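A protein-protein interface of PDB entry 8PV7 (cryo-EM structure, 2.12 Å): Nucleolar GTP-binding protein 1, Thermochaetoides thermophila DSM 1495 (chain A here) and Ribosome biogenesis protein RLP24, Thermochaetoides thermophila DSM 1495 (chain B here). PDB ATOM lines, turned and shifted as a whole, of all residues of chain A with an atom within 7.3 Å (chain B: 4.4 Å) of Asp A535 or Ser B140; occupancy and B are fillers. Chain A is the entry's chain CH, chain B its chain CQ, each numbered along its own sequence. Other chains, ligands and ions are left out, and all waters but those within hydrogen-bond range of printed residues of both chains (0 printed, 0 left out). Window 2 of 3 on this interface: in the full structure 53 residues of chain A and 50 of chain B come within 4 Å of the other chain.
The side-chain carboxylate of Asp A535 sits at hydrogen-bond distance from the backbone NH of Ser B140.
The guanidinium group of Arg B143 lies within salt-bridge range of the side-chain carboxylate of Asp A540, at 3.7 Å.
N of Gly B139 is in hydrogen-bond range of OD1 of Asp A535.
NH1 of Arg B138 is in salt-bridge range of OD2 of Asp A535, at 2.6 Å.
OD1 of Asp A532 lies within salt-bridge range of NH2 of Arg B138.
The side-chain hydroxyl (OG) of Ser B140 is in hydrogen-bond range of the side-chain carboxylate (OE1) of Glu B141.
Among the printed residues, merely in contact across the chains: Gln A536 with Arg B138, Gly A538 with Gly B139 and Glu A542 with Arg B143.
Gln A529 touches none of the printed residues of chain B.
Of the printed residues of chain B, Asp A532 touches Arg B138.
Asp A535 touches just these residues of chain B: Arg B138 (2.6 Å), Gly B139 (2.9 Å) and Ser B140 (3.1 Å).
Of the printed residues of chain B, Asp A540 touches Arg B143 (2.3 Å).
Of the printed residues of chain A, Gly B139 touches Asp A535 and Gly A538.
Ser B140 touches just one residue of chain A: Asp A535.
Arg B144 touches none of the printed residues of chain A.
The nearest residue of chain A that does not touch Ser B140 is Asp A540 (5.1 Å).
Of the 14 printed residues of chain A, 6 touch a printed residue of chain B.
Of the 7 printed residues of chain B, 4 touch a printed residue of chain A.
Along chain B the printed residues that touch a printed residue of chain A span positions 138 to 143.
Among the printed residues, Asp or Glu carboxylates within 4 Å of a Lys or Arg side-chain nitrogen of the other chain: Asp A532 with Arg B138, Asp A535 with Arg B138 and Asp A540 with Arg B143.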
ATOM      1  N   GLN A 529      18.780  23.292  -8.551  1.00  0.00           N
ATOM      2  CA  GLN A 529      19.031  23.700  -9.930  1.00  0.00           C
ATOM      3  C   GLN A 529      18.449  22.706 -10.926  1.00  0.00           C
ATOM      4  O   GLN A 529      17.873  23.106 -11.946  1.00  0.00           O
ATOM      5  CB  GLN A 529      20.529  23.873 -10.164  1.00  0.00           C
ATOM      6  CG  GLN A 529      21.217  24.750  -9.143  1.00  0.00           C
ATOM      7  CD  GLN A 529      22.493  25.363  -9.675  1.00  0.00           C
ATOM      8  OE1 GLN A 529      22.740  25.361 -10.880  1.00  0.00           O
ATOM      9  NE2 GLN A 529      23.318  25.886  -8.776  1.00  0.00           N
ATOM     10  N   LEU A 530      18.588  21.405 -10.649  1.00  0.00           N
ATOM     11  CA  LEU A 530      18.019  20.397 -11.542  1.00  0.00           C
ATOM     12  C   LEU A 530      16.497  20.496 -11.589  1.00  0.00           C
ATOM     13  O   LEU A 530      15.889  20.431 -12.668  1.00  0.00           O
ATOM     14  CB  LEU A 530      18.455  19.001 -11.103  1.00  0.00           C
ATOM     15  CG  LEU A 530      17.747  17.829 -11.785  1.00  0.00           C
ATOM     16  CD1 LEU A 530      18.070  17.780 -13.269  1.00  0.00           C
ATOM     17  CD2 LEU A 530      18.103  16.520 -11.109  1.00  0.00           C
ATOM     18  N   GLU A 531      15.871  20.676 -10.423  1.00  0.00           N
ATOM     19  CA  GLU A 531      14.422  20.829 -10.345  1.00  0.00           C
ATOM     20  C   GLU A 531      13.958  22.076 -11.082  1.00  0.00           C
ATOM     21  O   GLU A 531      12.956  22.041 -11.804  1.00  0.00           O
ATOM     22  CB  GLU A 531      13.988  20.876  -8.881  1.00  0.00           C
ATOM     23  CG  GLU A 531      12.641  20.243  -8.602  1.00  0.00           C
ATOM     24  CD  GLU A 531      11.493  21.195  -8.887  1.00  0.00           C
ATOM     25  OE1 GLU A 531      11.705  22.422  -8.802  1.00  0.00           O
ATOM     26  OE2 GLU A 531      10.380  20.720  -9.190  1.00  0.00           O
ATOM     27  N   ASP A 532      14.684  23.184 -10.919  1.00  0.00           N
ATOM     28  CA  ASP A 532      14.329  24.421 -11.604  1.00  0.00           C
ATOM     29  C   ASP A 532      14.417  24.260 -13.116  1.00  0.00           C
ATOM     30  O   ASP A 532      13.519  24.691 -13.849  1.00  0.00           O
ATOM     31  CB  ASP A 532      15.235  25.556 -11.129  1.00  0.00           C
ATOM     32  CG  ASP A 532      14.803  26.907 -11.655  1.00  0.00           C
ATOM     33  OD1 ASP A 532      13.619  27.058 -12.023  1.00  0.00           O
ATOM     34  OD2 ASP A 532      15.649  27.822 -11.706  1.00  0.00           O
ATOM     35  N   HIS A 533      15.487  23.621 -13.598  1.00  0.00           N
ATOM     36  CA  HIS A 533      15.660  23.449 -15.038  1.00  0.00           C
ATOM     37  C   HIS A 533      14.587  22.541 -15.624  1.00  0.00           C
ATOM     38  O   HIS A 533      14.038  22.824 -16.696  1.00  0.00           O
ATOM     39  CB  HIS A 533      17.051  22.897 -15.342  1.00  0.00           C
ATOM     40  CG  HIS A 533      17.325  22.744 -16.803  1.00  0.00           C
ATOM     41  ND1 HIS A 533      17.795  23.777 -17.583  1.00  0.00           N
ATOM     42  CD2 HIS A 533      17.181  21.683 -17.630  1.00  0.00           C
ATOM     43  CE1 HIS A 533      17.937  23.356 -18.827  1.00  0.00           C
ATOM     44  NE2 HIS A 533      17.572  22.089 -18.882  1.00  0.00           N
ATOM     45  N   LEU A 534      14.257  21.452 -14.925  1.00  0.00           N
ATOM     46  CA  LEU A 534      13.196  20.574 -15.408  1.00  0.00           C
ATOM     47  C   LEU A 534      11.838  21.267 -15.358  1.00  0.00           C
ATOM     48  O   LEU A 534      10.967  21.012 -16.200  1.00  0.00           O
ATOM     49  CB  LEU A 534      13.179  19.280 -14.600  1.00  0.00           C
ATOM     50  CG  LEU A 534      14.351  18.335 -14.869  1.00  0.00           C
ATOM     51  CD1 LEU A 534      14.185  17.047 -14.092  1.00  0.00           C
ATOM     52  CD2 LEU A 534      14.492  18.050 -16.355  1.00  0.00           C
ATOM     53  N   ASP A 535      11.648  22.167 -14.390  1.00  0.00           N
ATOM     54  CA  ASP A 535      10.407  22.928 -14.315  1.00  0.00           C
ATOM     55  C   ASP A 535      10.263  23.861 -15.512  1.00  0.00           C
ATOM     56  O   ASP A 535       9.200  23.916 -16.139  1.00  0.00           O
ATOM     57  CB  ASP A 535      10.357  23.713 -13.005  1.00  0.00           C
ATOM     58  CG  ASP A 535       8.957  24.172 -12.657  1.00  0.00           C
ATOM     59  OD1 ASP A 535       7.993  23.482 -13.045  1.00  0.00           O
ATOM     60  OD2 ASP A 535       8.820  25.224 -11.998  1.00  0.00           O
ATOM     61  N   GLN A 536      11.329  24.591 -15.858  1.00  0.00           N
ATOM     62  CA  GLN A 536      11.264  25.425 -17.059  1.00  0.00           C
ATOM     63  C   GLN A 536      11.155  24.602 -18.336  1.00  0.00           C
ATOM     64  O   GLN A 536      10.583  25.085 -19.318  1.00  0.00           O
ATOM     65  CB  GLN A 536      12.462  26.367 -17.173  1.00  0.00           C
ATOM     66  CG  GLN A 536      12.924  26.988 -15.886  1.00  0.00           C
ATOM     67  CD  GLN A 536      14.016  28.008 -16.103  1.00  0.00           C
ATOM     68  OE1 GLN A 536      14.048  28.694 -17.123  1.00  0.00           O
ATOM     69  NE2 GLN A 536      14.924  28.113 -15.141  1.00  0.00           N
ATOM     70  N   LEU A 537      11.675  23.378 -18.350  1.00  0.00           N
ATOM     71  CA  LEU A 537      11.413  22.474 -19.461  1.00  0.00           C
ATOM     72  C   LEU A 537      10.001  21.909 -19.439  1.00  0.00           C
ATOM     73  O   LEU A 537       9.586  21.278 -20.415  1.00  0.00           O
ATOM     74  CB  LEU A 537      12.424  21.326 -19.474  1.00  0.00           C
ATOM     75  CG  LEU A 537      13.861  21.704 -19.823  1.00  0.00           C
ATOM     76  CD1 LEU A 537      14.708  20.458 -19.892  1.00  0.00           C
ATOM     77  CD2 LEU A 537      13.912  22.462 -21.135  1.00  0.00           C
ATOM     78  N   GLY A 538       9.262  22.106 -18.351  1.00  0.00           N
ATOM     79  CA  GLY A 538       7.869  21.714 -18.326  1.00  0.00           C
ATOM     80  C   GLY A 538       7.636  20.301 -17.862  1.00  0.00           C
ATOM     81  O   GLY A 538       6.652  19.676 -18.266  1.00  0.00           O
ATOM     82  N   VAL A 539       8.516  19.780 -17.025  1.00  0.00           N
ATOM     83  CA  VAL A 539       8.435  18.415 -16.533  1.00  0.00           C
ATOM     84  C   VAL A 539       7.911  18.458 -15.108  1.00  0.00           C
ATOM     85  O   VAL A 539       8.401  19.230 -14.275  1.00  0.00           O
ATOM     86  CB  VAL A 539       9.812  17.726 -16.614  1.00  0.00           C
ATOM     87  CG1 VAL A 539       9.957  16.633 -15.562  1.00  0.00           C
ATOM     88  CG2 VAL A 539      10.041  17.174 -18.009  1.00  0.00           C
ATOM     89  N   ASP A 540       6.891  17.653 -14.833  1.00  0.00           N
ATOM     90  CA  ASP A 540       6.318  17.577 -13.493  1.00  0.00           C
ATOM     91  C   ASP A 540       7.237  16.731 -12.621  1.00  0.00           C
ATOM     92  O   ASP A 540       7.267  15.504 -12.734  1.00  0.00           O
ATOM     93  CB  ASP A 540       4.907  17.009 -13.548  1.00  0.00           C
ATOM     94  CG  ASP A 540       4.245  17.009 -12.203  1.00  0.00           C
ATOM     95  OD1 ASP A 540       3.767  15.949 -11.759  1.00  0.00           O
ATOM     96  OD2 ASP A 540       4.252  18.075 -11.568  1.00  0.00           O
ATOM     97  N   THR A 541       7.989  17.393 -11.740  1.00  0.00           N
ATOM     98  CA  THR A 541       9.039  16.707 -10.994  1.00  0.00           C
ATOM     99  C   THR A 541       8.488  15.980  -9.774  1.00  0.00           C
ATOM    100  O   THR A 541       9.138  15.073  -9.239  1.00  0.00           O
ATOM    101  CB  THR A 541      10.115  17.704 -10.571  1.00  0.00           C
ATOM    102  OG1 THR A 541       9.561  18.628  -9.628  1.00  0.00           O
ATOM    103  CG2 THR A 541      10.629  18.470 -11.775  1.00  0.00           C
ATOM    104  N   GLU A 542       7.302  16.368  -9.305  1.00  0.00           N
ATOM    105  CA  GLU A 542       6.750  15.727  -8.117  1.00  0.00           C
ATOM    106  C   GLU A 542       6.209  14.341  -8.435  1.00  0.00           C
ATOM    107  O   GLU A 542       6.164  13.470  -7.558  1.00  0.00           O
ATOM    108  CB  GLU A 542       5.664  16.604  -7.501  1.00  0.00           C
ATOM    109  CG  GLU A 542       6.096  18.038  -7.305  1.00  0.00           C
ATOM    110  CD  GLU A 542       6.611  18.313  -5.909  1.00  0.00           C
ATOM    111  OE1 GLU A 542       5.913  17.960  -4.936  1.00  0.00           O
ATOM    112  OE2 GLU A 542       7.713  18.886  -5.784  1.00  0.00           O
ATOM    113  N   ARG B 138       5.497  26.184 -16.921  1.00  0.00           N
ATOM    114  CA  ARG B 138       6.210  25.308 -16.005  1.00  0.00           C
ATOM    115  C   ARG B 138       5.328  24.138 -15.588  1.00  0.00           C
ATOM    116  O   ARG B 138       4.102  24.183 -15.710  1.00  0.00           O
ATOM    117  CB  ARG B 138       6.660  26.087 -14.772  1.00  0.00           C
ATOM    118  CG  ARG B 138       7.823  27.023 -15.018  1.00  0.00           C
ATOM    119  CD  ARG B 138       8.034  27.945 -13.834  1.00  0.00           C
ATOM    120  NE  ARG B 138       9.307  28.652 -13.901  1.00  0.00           N
ATOM    121  CZ  ARG B 138      10.424  28.237 -13.322  1.00  0.00           C
ATOM    122  NH1 ARG B 138      10.463  27.117 -12.620  1.00  0.00           N
ATOM    123  NH2 ARG B 138      11.529  28.967 -13.446  1.00  0.00           N
ATOM    124  N   GLY B 139       5.968  23.072 -15.102  1.00  0.00           N
ATOM    125  CA  GLY B 139       5.213  21.938 -14.592  1.00  0.00           C
ATOM    126  C   GLY B 139       4.412  22.285 -13.353  1.00  0.00           C
ATOM    127  O   GLY B 139       3.259  21.867 -13.206  1.00  0.00           O
ATOM    128  N   SER B 140       5.007  23.070 -12.451  1.00  0.00           N
ATOM    129  CA  SER B 140       4.282  23.541 -11.276  1.00  0.00           C
ATOM    130  C   SER B 140       3.147  24.481 -11.668  1.00  0.00           C
ATOM    131  O   SER B 140       2.079  24.476 -11.041  1.00  0.00           O
ATOM    132  CB  SER B 140       5.250  24.232 -10.316  1.00  0.00           C
ATOM    133  OG  SER B 140       5.916  25.303 -10.958  1.00  0.00           O
ATOM    134  N   GLU B 141       3.363  25.293 -12.706  1.00  0.00           N
ATOM    135  CA  GLU B 141       2.302  26.158 -13.211  1.00  0.00           C
ATOM    136  C   GLU B 141       1.154  25.339 -13.780  1.00  0.00           C
ATOM    137  O   GLU B 141      -0.017  25.669 -13.571  1.00  0.00           O
ATOM    138  CB  GLU B 141       2.858  27.114 -14.266  1.00  0.00           C
ATOM    139  CG  GLU B 141       3.775  28.205 -13.725  1.00  0.00           C
ATOM    140  CD  GLU B 141       3.567  28.484 -12.247  1.00  0.00           C
ATOM    141  OE1 GLU B 141       4.370  27.989 -11.427  1.00  0.00           O
ATOM    142  OE2 GLU B 141       2.605  29.204 -11.906  1.00  0.00           O
ATOM    143  N   LYS B 142       1.472  24.259 -14.498  1.00  0.00           N
ATOM    144  CA  LYS B 142       0.428  23.376 -15.010  1.00  0.00           C
ATOM    145  C   LYS B 142      -0.323  22.693 -13.876  1.00  0.00           C
ATOM    146  O   LYS B 142      -1.542  22.510 -13.957  1.00  0.00           O
ATOM    147  CB  LYS B 142       1.022  22.338 -15.959  1.00  0.00           C
ATOM    148  CG  LYS B 142       1.504  22.900 -17.282  1.00  0.00           C
ATOM    149  CD  LYS B 142       1.772  21.781 -18.275  1.00  0.00           C
ATOM    150  CE  LYS B 142       2.339  22.310 -19.583  1.00  0.00           C
ATOM    151  NZ  LYS B 142       3.733  22.818 -19.425  1.00  0.00           N
ATOM    152  N   ARG B 143       0.389  22.319 -12.807  1.00  0.00           N
ATOM    153  CA  ARG B 143      -0.262  21.768 -11.618  1.00  0.00           C
ATOM    154  C   ARG B 143      -1.259  22.751 -11.017  1.00  0.00           C
ATOM    155  O   ARG B 143      -2.413  22.394 -10.738  1.00  0.00           O
ATOM    156  CB  ARG B 143       0.779  21.413 -10.562  1.00  0.00           C
ATOM    157  CG  ARG B 143       0.632  20.048  -9.940  1.00  0.00           C
ATOM    158  CD  ARG B 143       1.989  19.428  -9.832  1.00  0.00           C
ATOM    159  NE  ARG B 143       2.829  20.195  -8.921  1.00  0.00           N
ATOM    160  CZ  ARG B 143       4.146  20.306  -9.026  1.00  0.00           C
ATOM    161  NH1 ARG B 143       4.816  19.709  -9.997  1.00  0.00           N
ATOM    162  NH2 ARG B 143       4.808  21.041  -8.137  1.00  0.00           N
ATOM    163  N   ARG B 144      -0.820  23.993 -10.793  1.00  0.00           N
ATOM    164  CA  ARG B 144      -1.689  24.958 -10.129  1.00  0.00           C
ATOM    165  C   ARG B 144      -2.850  25.362 -11.033  1.00  0.00           C
ATOM    166  O   ARG B 144      -3.970  25.572 -10.555  1.00  0.00           O
ATOM    167  CB  ARG B 144      -0.882  26.169  -9.645  1.00  0.00           C
ATOM    168  CG  ARG B 144      -0.608  27.261 -10.658  1.00  0.00           C
ATOM    169  CD  ARG B 144      -0.405  28.598  -9.971  1.00  0.00           C
ATOM    170  NE  ARG B 144      -0.391  29.698 -10.925  1.00  0.00           N
ATOM    171  CZ  ARG B 144      -0.277  30.977 -10.593  1.00  0.00           C
ATOM    172  NH1 ARG B 144      -0.158  31.354  -9.330  1.00  0.00           N
ATOM    173  NH2 ARG B 144      -0.280  31.899 -11.550  1.00  0.00           N
